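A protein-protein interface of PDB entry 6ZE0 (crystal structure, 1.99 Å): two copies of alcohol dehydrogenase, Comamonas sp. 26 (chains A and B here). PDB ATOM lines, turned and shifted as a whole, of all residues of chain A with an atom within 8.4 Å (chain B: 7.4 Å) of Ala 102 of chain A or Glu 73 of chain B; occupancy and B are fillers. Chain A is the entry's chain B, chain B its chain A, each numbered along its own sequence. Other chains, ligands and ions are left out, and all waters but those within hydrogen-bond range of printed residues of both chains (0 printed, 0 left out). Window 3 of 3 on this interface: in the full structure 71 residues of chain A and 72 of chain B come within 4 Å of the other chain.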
ATOM      1  N   PHE A  97      29.861 -12.644  31.768  1.00  0.00           N
ATOM      2  CA  PHE A  97      28.540 -12.030  31.681  1.00  0.00           C
ATOM      3  C   PHE A  97      28.631 -10.508  31.660  1.00  0.00           C
ATOM      4  O   PHE A  97      27.920  -9.849  30.893  1.00  0.00           O
ATOM      5  CB  PHE A  97      27.660 -12.498  32.837  1.00  0.00           C
ATOM      6  CG  PHE A  97      26.240 -12.024  32.742  1.00  0.00           C
ATOM      7  CD1 PHE A  97      25.349 -12.636  31.872  1.00  0.00           C
ATOM      8  CD2 PHE A  97      25.791 -10.968  33.517  1.00  0.00           C
ATOM      9  CE1 PHE A  97      24.038 -12.206  31.780  1.00  0.00           C
ATOM     10  CE2 PHE A  97      24.483 -10.535  33.431  1.00  0.00           C
ATOM     11  CZ  PHE A  97      23.604 -11.152  32.560  1.00  0.00           C
ATOM     12  N   GLN A  99      30.766  -8.692  30.403  1.00  0.00           N
ATOM     13  CA  GLN A  99      31.262  -8.221  29.117  1.00  0.00           C
ATOM     14  C   GLN A  99      30.225  -8.328  28.009  1.00  0.00           C
ATOM     15  O   GLN A  99      30.526  -7.975  26.864  1.00  0.00           O
ATOM     16  CB  GLN A  99      32.520  -8.997  28.711  1.00  0.00           C
ATOM     17  CG  GLN A  99      33.700  -8.805  29.643  1.00  0.00           C
ATOM     18  CD  GLN A  99      34.895  -9.646  29.241  1.00  0.00           C
ATOM     19  OE1 GLN A  99      34.748 -10.687  28.602  1.00  0.00           O
ATOM     20  NE2 GLN A  99      36.087  -9.195  29.609  1.00  0.00           N
ATOM     21  N   GLN A 100      29.019  -8.797  28.312  1.00  0.00           N
ATOM     22  CA  GLN A 100      28.019  -8.977  27.275  1.00  0.00           C
ATOM     23  C   GLN A 100      27.337  -7.652  26.948  1.00  0.00           C
ATOM     24  O   GLN A 100      27.324  -6.710  27.746  1.00  0.00           O
ATOM     25  CB  GLN A 100      26.975 -10.011  27.698  1.00  0.00           C
ATOM     26  CG  GLN A 100      27.541 -11.400  27.939  1.00  0.00           C
ATOM     27  CD  GLN A 100      28.437 -11.867  26.809  1.00  0.00           C
ATOM     28  OE1 GLN A 100      28.041 -11.862  25.642  1.00  0.00           O
ATOM     29  NE2 GLN A 100      29.655 -12.275  27.150  1.00  0.00           N
ATOM     30  N   ASN A 101      26.761  -7.599  25.752  1.00  0.00           N
ATOM     31  CA  ASN A 101      26.106  -6.415  25.222  1.00  0.00           C
ATOM     32  C   ASN A 101      24.625  -6.703  25.026  1.00  0.00           C
ATOM     33  O   ASN A 101      24.206  -7.858  24.927  1.00  0.00           O
ATOM     34  CB  ASN A 101      26.740  -5.994  23.885  1.00  0.00           C
ATOM     35  CG  ASN A 101      26.365  -4.588  23.471  1.00  0.00           C
ATOM     36  OD1 ASN A 101      25.434  -3.994  24.015  1.00  0.00           O
ATOM     37  ND2 ASN A 101      27.080  -4.050  22.491  1.00  0.00           N
ATOM     38  N   ALA A 102      23.827  -5.634  24.965  1.00  0.00           N
ATOM     39  CA  ALA A 102      22.428  -5.797  24.586  1.00  0.00           C
ATOM     40  C   ALA A 102      22.317  -6.399  23.193  1.00  0.00           C
ATOM     41  O   ALA A 102      21.453  -7.248  22.939  1.00  0.00           O
ATOM     42  CB  ALA A 102      21.699  -4.455  24.658  1.00  0.00           C
ATOM     43  N   GLN A 103      23.188  -5.968  22.277  1.00  0.00           N
ATOM     44  CA  GLN A 103      23.223  -6.549  20.938  1.00  0.00           C
ATOM     45  C   GLN A 103      23.646  -8.013  20.980  1.00  0.00           C
ATOM     46  O   GLN A 103      23.039  -8.864  20.319  1.00  0.00           O
ATOM     47  CB  GLN A 103      24.168  -5.741  20.046  1.00  0.00           C
ATOM     48  CG  GLN A 103      24.377  -6.333  18.663  1.00  0.00           C
ATOM     49  CD  GLN A 103      25.437  -5.596  17.868  1.00  0.00           C
ATOM     50  OE1 GLN A 103      25.965  -4.575  18.311  1.00  0.00           O
ATOM     51  NE2 GLN A 103      25.756  -6.112  16.685  1.00  0.00           N
ATOM     52  N   SER A 104      24.692  -8.327  21.751  1.00  0.00           N
ATOM     53  CA  SER A 104      25.183  -9.701  21.811  1.00  0.00           C
ATOM     54  C   SER A 104      24.172 -10.629  22.474  1.00  0.00           C
ATOM     55  O   SER A 104      23.998 -11.775  22.042  1.00  0.00           O
ATOM     56  CB  SER A 104      26.520  -9.755  22.550  1.00  0.00           C
ATOM     57  OG  SER A 104      26.358  -9.465  23.928  1.00  0.00           O
ATOM     58  N   ILE A 105      23.499 -10.157  23.527  1.00  0.00           N
ATOM     59  CA  ILE A 105      22.506 -10.987  24.206  1.00  0.00           C
ATOM     60  C   ILE A 105      21.334 -11.283  23.282  1.00  0.00           C
ATOM     61  O   ILE A 105      20.846 -12.418  23.221  1.00  0.00           O
ATOM     62  CB  ILE A 105      22.043 -10.311  25.509  1.00  0.00           C
ATOM     63  CG1 ILE A 105      23.185 -10.265  26.524  1.00  0.00           C
ATOM     64  CG2 ILE A 105      20.840 -11.033  26.091  1.00  0.00           C
ATOM     65  CD1 ILE A 105      22.907  -9.356  27.697  1.00  0.00           C
ATOM     66  N   ASP A 106      20.862 -10.267  22.554  1.00  0.00           N
ATOM     67  CA  ASP A 106      19.766 -10.465  21.610  1.00  0.00           C
ATOM     68  C   ASP A 106      20.098 -11.552  20.596  1.00  0.00           C
ATOM     69  O   ASP A 106      19.307 -12.477  20.381  1.00  0.00           O
ATOM     70  CB  ASP A 106      19.443  -9.150  20.897  1.00  0.00           C
ATOM     71  CG  ASP A 106      18.554  -8.243  21.720  1.00  0.00           C
ATOM     72  OD1 ASP A 106      18.208  -8.622  22.857  1.00  0.00           O
ATOM     73  OD2 ASP A 106      18.197  -7.152  21.230  1.00  0.00           O
ATOM     74  N   ARG A 107      21.274 -11.459  19.968  1.00  0.00           N
ATOM     75  CA  ARG A 107      21.644 -12.418  18.931  1.00  0.00           C
ATOM     76  C   ARG A 107      21.831 -13.818  19.504  1.00  0.00           C
ATOM     77  O   ARG A 107      21.433 -14.807  18.878  1.00  0.00           O
ATOM     78  CB  ARG A 107      22.917 -11.957  18.221  1.00  0.00           C
ATOM     79  CG  ARG A 107      22.778 -10.625  17.500  1.00  0.00           C
ATOM     80  CD  ARG A 107      24.078 -10.227  16.818  1.00  0.00           C
ATOM     81  NE  ARG A 107      24.582 -11.289  15.951  1.00  0.00           N
ATOM     82  CZ  ARG A 107      24.208 -11.462  14.688  1.00  0.00           C
ATOM     83  NH1 ARG A 107      23.322 -10.641  14.138  1.00  0.00           N
ATOM     84  NH2 ARG A 107      24.718 -12.456  13.974  1.00  0.00           N
ATOM     85  N   LEU A 108      22.433 -13.922  20.690  1.00  0.00           N
ATOM     86  CA  LEU A 108      22.673 -15.232  21.289  1.00  0.00           C
ATOM     87  C   LEU A 108      21.362 -15.946  21.602  1.00  0.00           C
ATOM     88  O   LEU A 108      21.200 -17.134  21.298  1.00  0.00           O
ATOM     89  CB  LEU A 108      23.522 -15.072  22.552  1.00  0.00           C
ATOM     90  CG  LEU A 108      24.031 -16.340  23.238  1.00  0.00           C
ATOM     91  CD1 LEU A 108      24.641 -17.295  22.232  1.00  0.00           C
ATOM     92  CD2 LEU A 108      25.046 -15.977  24.314  1.00  0.00           C
ATOM     93  N   VAL A 109      20.416 -15.239  22.222  1.00  0.00           N
ATOM     94  CA  VAL A 109      19.113 -15.836  22.495  1.00  0.00           C
ATOM     95  C   VAL A 109      18.361 -16.107  21.197  1.00  0.00           C
ATOM     96  O   VAL A 109      17.773 -17.180  21.017  1.00  0.00           O
ATOM     97  CB  VAL A 109      18.299 -14.932  23.437  1.00  0.00           C
ATOM     98  CG1 VAL A 109      16.925 -15.537  23.692  1.00  0.00           C
ATOM     99  CG2 VAL A 109      19.051 -14.714  24.745  1.00  0.00           C
ATOM    100  N   LEU B   8      13.993  -2.108  41.885  1.00  0.00           N
ATOM    101  CA  LEU B   8      13.294  -2.064  40.609  1.00  0.00           C
ATOM    102  C   LEU B   8      12.625  -3.411  40.380  1.00  0.00           C
ATOM    103  O   LEU B   8      13.278  -4.457  40.456  1.00  0.00           O
ATOM    104  CB  LEU B   8      14.247  -1.727  39.461  1.00  0.00           C
ATOM    105  CG  LEU B   8      13.584  -1.448  38.107  1.00  0.00           C
ATOM    106  CD1 LEU B   8      14.301  -0.330  37.373  1.00  0.00           C
ATOM    107  CD2 LEU B   8      13.549  -2.702  37.241  1.00  0.00           C
ATOM    108  N   LEU B  63       8.236  -4.924  27.912  1.00  0.00           N
ATOM    109  CA  LEU B  63       9.582  -5.462  27.770  1.00  0.00           C
ATOM    110  C   LEU B  63       9.747  -6.351  26.545  1.00  0.00           C
ATOM    111  O   LEU B  63      10.850  -6.864  26.323  1.00  0.00           O
ATOM    112  CB  LEU B  63       9.970  -6.219  29.041  1.00  0.00           C
ATOM    113  CG  LEU B  63      10.111  -5.298  30.255  1.00  0.00           C
ATOM    114  CD1 LEU B  63      10.516  -6.068  31.500  1.00  0.00           C
ATOM    115  CD2 LEU B  63      11.115  -4.192  29.961  1.00  0.00           C
ATOM    116  N   GLN B  66      11.813  -3.024  22.014  1.00  0.00           N
ATOM    117  CA  GLN B  66      13.214  -2.642  22.166  1.00  0.00           C
ATOM    118  C   GLN B  66      13.352  -1.304  22.880  1.00  0.00           C
ATOM    119  O   GLN B  66      14.261  -1.125  23.699  1.00  0.00           O
ATOM    120  CB  GLN B  66      13.904  -2.604  20.802  1.00  0.00           C
ATOM    121  CG  GLN B  66      14.027  -3.968  20.136  1.00  0.00           C
ATOM    122  CD  GLN B  66      14.990  -4.896  20.862  1.00  0.00           C
ATOM    123  OE1 GLN B  66      15.840  -4.451  21.635  1.00  0.00           O
ATOM    124  NE2 GLN B  66      14.860  -6.193  20.611  1.00  0.00           N
ATOM    125  N   LYS B  67      12.468  -0.350  22.580  1.00  0.00           N
ATOM    126  CA  LYS B  67      12.548   0.958  23.224  1.00  0.00           C
ATOM    127  C   LYS B  67      12.322   0.846  24.725  1.00  0.00           C
ATOM    128  O   LYS B  67      13.090   1.398  25.522  1.00  0.00           O
ATOM    129  CB  LYS B  67      11.522   1.916  22.621  1.00  0.00           C
ATOM    130  CG  LYS B  67      11.490   3.251  23.351  1.00  0.00           C
ATOM    131  CD  LYS B  67      10.306   4.102  22.949  1.00  0.00           C
ATOM    132  CE  LYS B  67      10.302   5.417  23.709  1.00  0.00           C
ATOM    133  NZ  LYS B  67       9.164   6.287  23.313  1.00  0.00           N
ATOM    134  N   ASP B  68      11.264   0.139  25.128  1.00  0.00           N
ATOM    135  CA  ASP B  68      10.956   0.021  26.549  1.00  0.00           C
ATOM    136  C   ASP B  68      12.064  -0.710  27.293  1.00  0.00           C
ATOM    137  O   ASP B  68      12.466  -0.295  28.387  1.00  0.00           O
ATOM    138  CB  ASP B  68       9.621  -0.699  26.743  1.00  0.00           C
ATOM    139  CG  ASP B  68       8.493  -0.064  25.949  1.00  0.00           C
ATOM    140  OD1 ASP B  68       8.778   0.781  25.074  1.00  0.00           O
ATOM    141  OD2 ASP B  68       7.319  -0.406  26.206  1.00  0.00           O
ATOM    142  N   LEU B  69      12.568  -1.803  26.715  1.00  0.00           N
ATOM    143  CA  LEU B  69      13.636  -2.560  27.359  1.00  0.00           C
ATOM    144  C   LEU B  69      14.902  -1.722  27.498  1.00  0.00           C
ATOM    145  O   LEU B  69      15.579  -1.776  28.532  1.00  0.00           O
ATOM    146  CB  LEU B  69      13.912  -3.840  26.568  1.00  0.00           C
ATOM    147  CG  LEU B  69      14.948  -4.802  27.141  1.00  0.00           C
ATOM    148  CD1 LEU B  69      14.635  -5.117  28.595  1.00  0.00           C
ATOM    149  CD2 LEU B  69      14.978  -6.073  26.320  1.00  0.00           C
ATOM    150  N   ALA B  70      15.237  -0.938  26.468  1.00  0.00           N
ATOM    151  CA  ALA B  70      16.416  -0.079  26.537  1.00  0.00           C
ATOM    152  C   ALA B  70      16.259   1.019  27.581  1.00  0.00           C
ATOM    153  O   ALA B  70      17.248   1.434  28.195  1.00  0.00           O
ATOM    154  CB  ALA B  70      16.704   0.534  25.167  1.00  0.00           C
ATOM    155  N   GLU B  71      15.034   1.509  27.786  1.00  0.00           N
ATOM    156  CA  GLU B  71      14.809   2.532  28.801  1.00  0.00           C
ATOM    157  C   GLU B  71      15.025   1.979  30.204  1.00  0.00           C
ATOM    158  O   GLU B  71      15.608   2.654  31.061  1.00  0.00           O
ATOM    159  CB  GLU B  71      13.401   3.111  28.654  1.00  0.00           C
ATOM    160  CG  GLU B  71      13.044   4.170  29.686  1.00  0.00           C
ATOM    161  CD  GLU B  71      11.640   4.715  29.500  1.00  0.00           C
ATOM    162  OE1 GLU B  71      10.961   4.298  28.537  1.00  0.00           O
ATOM    163  OE2 GLU B  71      11.217   5.564  30.314  1.00  0.00           O
ATOM    164  N   VAL B  72      14.565   0.752  30.459  1.00  0.00           N
ATOM    165  CA  VAL B  72      14.746   0.157  31.780  1.00  0.00           C
ATOM    166  C   VAL B  72      16.212  -0.191  32.014  1.00  0.00           C
ATOM    167  O   VAL B  72      16.728  -0.041  33.130  1.00  0.00           O
ATOM    168  CB  VAL B  72      13.835  -1.074  31.940  1.00  0.00           C
ATOM    169  CG1 VAL B  72      13.993  -1.683  33.328  1.00  0.00           C
ATOM    170  CG2 VAL B  72      12.384  -0.692  31.688  1.00  0.00           C
ATOM    171  N   GLU B  73      16.905  -0.663  30.974  1.00  0.00           N
ATOM    172  CA  GLU B  73      18.342  -0.898  31.079  1.00  0.00           C
ATOM    173  C   GLU B  73      19.074   0.373  31.484  1.00  0.00           C
ATOM    174  O   GLU B  73      19.929   0.357  32.377  1.00  0.00           O
ATOM    175  CB  GLU B  73      18.887  -1.422  29.750  1.00  0.00           C
ATOM    176  CG  GLU B  73      18.485  -2.842  29.406  1.00  0.00           C
ATOM    177  CD  GLU B  73      18.920  -3.236  28.007  1.00  0.00           C
ATOM    178  OE1 GLU B  73      18.699  -2.440  27.070  1.00  0.00           O
ATOM    179  OE2 GLU B  73      19.487  -4.338  27.843  1.00  0.00           O
ATOM    180  N   THR B  74      18.749   1.491  30.827  1.00  0.00           N
ATOM    181  CA  THR B  74      19.397   2.761  31.142  1.00  0.00           C
ATOM    182  C   THR B  74      19.126   3.178  32.581  1.00  0.00           C
ATOM    183  O   THR B  74      20.026   3.675  33.270  1.00  0.00           O
ATOM    184  CB  THR B  74      18.927   3.838  30.168  1.00  0.00           C
ATOM    185  OG1 THR B  74      19.276   3.455  28.832  1.00  0.00           O
ATOM    186  CG2 THR B  74      19.569   5.180  30.494  1.00  0.00           C
ATOM    187  N   ARG B  75      17.888   2.995  33.047  1.00  0.00           N
ATOM    188  CA  ARG B  75      17.569   3.304  34.438  1.00  0.00           C
ATOM    189  C   ARG B  75      18.391   2.450  35.392  1.00  0.00           C
ATOM    190  O   ARG B  75      18.920   2.952  36.390  1.00  0.00           O
ATOM    191  CB  ARG B  75      16.075   3.105  34.695  1.00  0.00           C
ATOM    192  CG  ARG B  75      15.637   3.469  36.105  1.00  0.00           C
ATOM    193  CD  ARG B  75      15.957   4.925  36.413  1.00  0.00           C
ATOM    194  NE  ARG B  75      15.534   5.310  37.756  1.00  0.00           N
ATOM    195  CZ  ARG B  75      14.355   5.852  38.041  1.00  0.00           C
ATOM    196  NH1 ARG B  75      13.477   6.075  37.073  1.00  0.00           N
ATOM    197  NH2 ARG B  75      14.054   6.172  39.291  1.00  0.00           N
ATOM    198  N   LEU B  76      18.523   1.156  35.093  1.00  0.00           N
ATOM    199  CA  LEU B  76      19.276   0.259  35.963  1.00  0.00           C
ATOM    200  C   LEU B  76      20.763   0.596  35.967  1.00  0.00           C
ATOM    201  O   LEU B  76      21.431   0.470  37.001  1.00  0.00           O
ATOM    202  CB  LEU B  76      19.062  -1.190  35.527  1.00  0.00           C
ATOM    203  CG  LEU B  76      17.694  -1.810  35.803  1.00  0.00           C
ATOM    204  CD1 LEU B  76      17.584  -3.165  35.122  1.00  0.00           C
ATOM    205  CD2 LEU B  76      17.469  -1.945  37.299  1.00  0.00           C
ATOM    206  N   ARG B  77      21.299   1.030  34.824  1.00  0.00           N
ATOM    207  CA  ARG B  77      22.727   1.319  34.743  1.00  0.00           C
ATOM    208  C   ARG B  77      23.081   2.597  35.493  1.00  0.00           C
ATOM    209  O   ARG B  77      24.102   2.652  36.188  1.00  0.00           O
ATOM    210  CB  ARG B  77      23.161   1.433  33.281  1.00  0.00           C
ATOM    211  CG  ARG B  77      23.611   0.133  32.647  1.00  0.00           C
ATOM    212  CD  ARG B  77      24.254   0.394  31.295  1.00  0.00           C
ATOM    213  NE  ARG B  77      23.318   1.034  30.374  1.00  0.00           N
ATOM    214  CZ  ARG B  77      22.562   0.376  29.500  1.00  0.00           C
ATOM    215  NH1 ARG B  77      22.633  -0.946  29.422  1.00  0.00           N
ATOM    216  NH2 ARG B  77      21.736   1.039  28.703  1.00  0.00           N
ATOM    217  N   GLU B  78      22.250   3.629  35.366  1.00  0.00           N
ATOM    218  CA  GLU B  78      22.608   4.961  35.836  1.00  0.00           C
ATOM    219  C   GLU B  78      22.113   5.260  37.245  1.00  0.00           C
ATOM    220  O   GLU B  78      22.742   6.052  37.955  1.00  0.00           O
ATOM    221  CB  GLU B  78      22.061   6.012  34.867  1.00  0.00           C
ATOM    222  CG  GLU B  78      22.642   5.901  33.462  1.00  0.00           C
ATOM    223  CD  GLU B  78      22.119   6.972  32.522  1.00  0.00           C
ATOM    224  OE1 GLU B  78      21.152   7.672  32.890  1.00  0.00           O
ATOM    225  OE2 GLU B  78      22.672   7.108  31.411  1.00  0.00           O
ATOM    226  N   ASP B  79      21.020   4.639  37.679  1.00  0.00           N
ATOM    227  CA  ASP B  79      20.464   4.910  39.004  1.00  0.00           C
ATOM    228  C   ASP B  79      21.270   4.132  40.035  1.00  0.00           C
ATOM    229  O   ASP B  79      21.017   2.949  40.279  1.00  0.00           O
ATOM    230  CB  ASP B  79      18.988   4.535  39.058  1.00  0.00           C
ATOM    231  CG  ASP B  79      18.285   5.083  40.287  1.00  0.00           C
ATOM    232  OD1 ASP B  79      18.963   5.385  41.292  1.00  0.00           O
ATOM    233  OD2 ASP B  79      17.042   5.205  40.248  1.00  0.00           O
ATOM    234  N   THR B 114      14.959 -13.102  27.078  1.00  0.00           N
ATOM    235  CA  THR B 114      15.822 -12.015  26.623  1.00  0.00           C
ATOM    236  C   THR B 114      15.776 -10.832  27.581  1.00  0.00           C
ATOM    237  O   THR B 114      16.821 -10.322  28.002  1.00  0.00           O
ATOM    238  CB  THR B 114      15.421 -11.576  25.214  1.00  0.00           C
ATOM    239  OG1 THR B 114      15.406 -12.712  24.340  1.00  0.00           O
ATOM    240  CG2 THR B 114      16.405 -10.550  24.681  1.00  0.00           C
ATOM    241  N   ALA B 115      14.571 -10.379  27.936  1.00  0.00           N
ATOM    242  CA  ALA B 115      14.441  -9.215  28.811  1.00  0.00           C
ATOM    243  C   ALA B 115      15.099  -9.412  30.173  1.00  0.00           C
ATOM    244  O   ALA B 115      15.890  -8.541  30.577  1.00  0.00           O
ATOM    245  CB  ALA B 115      12.962  -8.835  28.944  1.00  0.00           C
ATOM    246  N   THR B 117      17.512 -11.396  31.058  1.00  0.00           N
ATOM    247  CA  THR B 117      18.954 -11.487  30.852  1.00  0.00           C
ATOM    248  C   THR B 117      19.562 -10.112  30.610  1.00  0.00           C
ATOM    249  O   THR B 117      20.630  -9.792  31.145  1.00  0.00           O
ATOM    250  CB  THR B 117      19.258 -12.416  29.675  1.00  0.00           C
ATOM    251  OG1 THR B 117      18.660 -13.698  29.908  1.00  0.00           O
ATOM    252  CG2 THR B 117      20.765 -12.587  29.500  1.00  0.00           C
ATOM    253  N   ARG B 118      18.893  -9.284  29.805  1.00  0.00           N
ATOM    254  CA  ARG B 118      19.424  -7.958  29.508  1.00  0.00           C
ATOM    255  C   ARG B 118      19.362  -7.047  30.729  1.00  0.00           C
ATOM    256  O   ARG B 118      20.270  -6.236  30.949  1.00  0.00           O
ATOM    257  CB  ARG B 118      18.672  -7.349  28.325  1.00  0.00           C
ATOM    258  CG  ARG B 118      19.198  -7.825  26.976  1.00  0.00           C
ATOM    259  CD  ARG B 118      18.375  -7.300  25.810  1.00  0.00           C
ATOM    260  NE  ARG B 118      18.366  -5.842  25.740  1.00  0.00           N
ATOM    261  CZ  ARG B 118      17.864  -5.149  24.722  1.00  0.00           C
ATOM    262  NH1 ARG B 118      17.331  -5.783  23.685  1.00  0.00           N
ATOM    263  NH2 ARG B 118      17.892  -3.824  24.739  1.00  0.00           N
ATOM    264  N   LEU B 119      18.302  -7.161  31.532  1.00  0.00           N
ATOM    265  CA  LEU B 119      18.206  -6.347  32.740  1.00  0.00           C
ATOM    266  C   LEU B 119      19.255  -6.758  33.768  1.00  0.00           C
ATOM    267  O   LEU B 119      19.834  -5.904  34.447  1.00  0.00           O
ATOM    268  CB  LEU B 119      16.799  -6.440  33.330  1.00  0.00           C
ATOM    269  CG  LEU B 119      15.706  -5.814  32.459  1.00  0.00           C
ATOM    270  CD1 LEU B 119      14.370  -5.781  33.193  1.00  0.00           C
ATOM    271  CD2 LEU B 119      16.112  -4.420  31.988  1.00  0.00           C
ATOM    272  N   ALA B 120      19.503  -8.064  33.902  1.00  0.00           N
ATOM    273  CA  ALA B 120      20.587  -8.523  34.765  1.00  0.00           C
ATOM    274  C   ALA B 120      21.930  -7.987  34.287  1.00  0.00           C
ATOM    275  O   ALA B 120      22.784  -7.612  35.099  1.00  0.00           O
ATOM    276  CB  ALA B 120      20.603 -10.050  34.827  1.00  0.00           C
ATOM    277  N   ALA B 121      22.139  -7.949  32.968  1.00  0.00           N
ATOM    278  CA  ALA B 121      23.392  -7.430  32.431  1.00  0.00           C
ATOM    279  C   ALA B 121      23.540  -5.938  32.691  1.00  0.00           C
ATOM    280  O   ALA B 121      24.660  -5.452  32.887  1.00  0.00           O
ATOM    281  CB  ALA B 121      23.488  -7.720  30.934  1.00  0.00           C
ATOM    282  N   ALA B 122      22.430  -5.197  32.682  1.00  0.00           N
ATOM    283  CA  ALA B 122      22.495  -3.760  32.919  1.00  0.00           C
ATOM    284  C   ALA B 122      22.980  -3.444  34.331  1.00  0.00           C
ATOM    285  O   ALA B 122      23.721  -2.476  34.536  1.00  0.00           O
ATOM    286  CB  ALA B 122      21.126  -3.129  32.665  1.00  0.00           C
ATOM    287  N   VAL B 123      22.571  -4.240  35.317  1.00  0.00           N
ATOM    288  CA  VAL B 123      22.973  -3.982  36.697  1.00  0.00           C
ATOM    289  C   VAL B 123      24.304  -4.632  37.064  1.00  0.00           C
ATOM    290  O   VAL B 123      25.008  -4.130  37.946  1.00  0.00           O
ATOM    291  CB  VAL B 123      21.876  -4.427  37.679  1.00  0.00           C
ATOM    292  CG1 VAL B 123      20.721  -3.450  37.665  1.00  0.00           C
ATOM    293  CG2 VAL B 123      21.402  -5.835  37.354  1.00  0.00           C
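NH1 of Arg 118 of chain B lies within salt-bridge range of OD2 of Asp 106 of chain A (2.9 Å).
NE of Arg 118 of chain B lies within salt-bridge range of OE2 of Glu 73 of chain B. The guanidinium group (NH1) of Arg 118 of chain B lies within hydrogen-bond range of the side-chain amide oxygen (OE1) of Gln 66 of chain B, 2.9 Å away.
Among the printed residues, merely in contact across the chains: Phe 97 of chain A with Thr 117 of chain B, Phe 97 of chain A with Ala 120 of chain B, Phe 97 of chain A with Ala 121 of chain B, Ala 102 of chain A with Glu 73 of chain B, Ala 102 of chain A with Arg 118 of chain B, Ile 105 of chain A with Thr 117 of chain B, Ile 105 of chain A with Arg 118 of chain B, Ile 105 of chain A with Ala 121 of chain B, Asp 106 of chain A with Gln 66 of chain B, Asp 106 of chain A with Thr 114 of chain B and Val 109 of chain A with Thr 114 of chain B.
Ala 102 of chain A touches just these residues of chain B: Glu 73 (3.9 Å) and Arg 118 (3.8 Å). Glu 73 of chain B touches one residue of chain A. No residue of chain A comes within 4 Å of Ala 70 of chain B. Of the printed residues of chain A, Ala 121 of chain B touches Phe 97 and Ile 105. Printed residues of chain A within 4 Å of Arg 118 of chain B: Ala 102 (3.8 Å), Ile 105 (3.7 Å) and Asp 106 (2.9 Å). Of the printed residues of chain A, Thr 117 of chain B touches Phe 97 (3.6 Å) and Ile 105 (3.7 Å). Leu 119 of chain B touches none of the printed residues of chain A. The nearest printed residue of chain A that does not touch Ala 120 of chain B is Ile 105 of chain A (6.8 Å).
Hydrophobic or aromatic side chains of chain B that line the printed part of chain A: Ala 120 and Ala 121. Along chain B the printed residues that touch a printed residue of chain A span positions 66 to 121. Of the 12 printed residues of chain A, 5 touch a printed residue of chain B. Printed residues of chain A that touch a printed residue of chain B: Phe 97, Ala 102, Ile 105, Asp 106 and Val 109. Among the printed residues, 12 pairs touch across the chains. Among the printed residues, Asp or Glu carboxylates within 4 Å of a Lys or Arg side-chain nitrogen of the other chain: Asp 106 of chain A with Arg 118 of chain B.
No position is printed for both chains.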
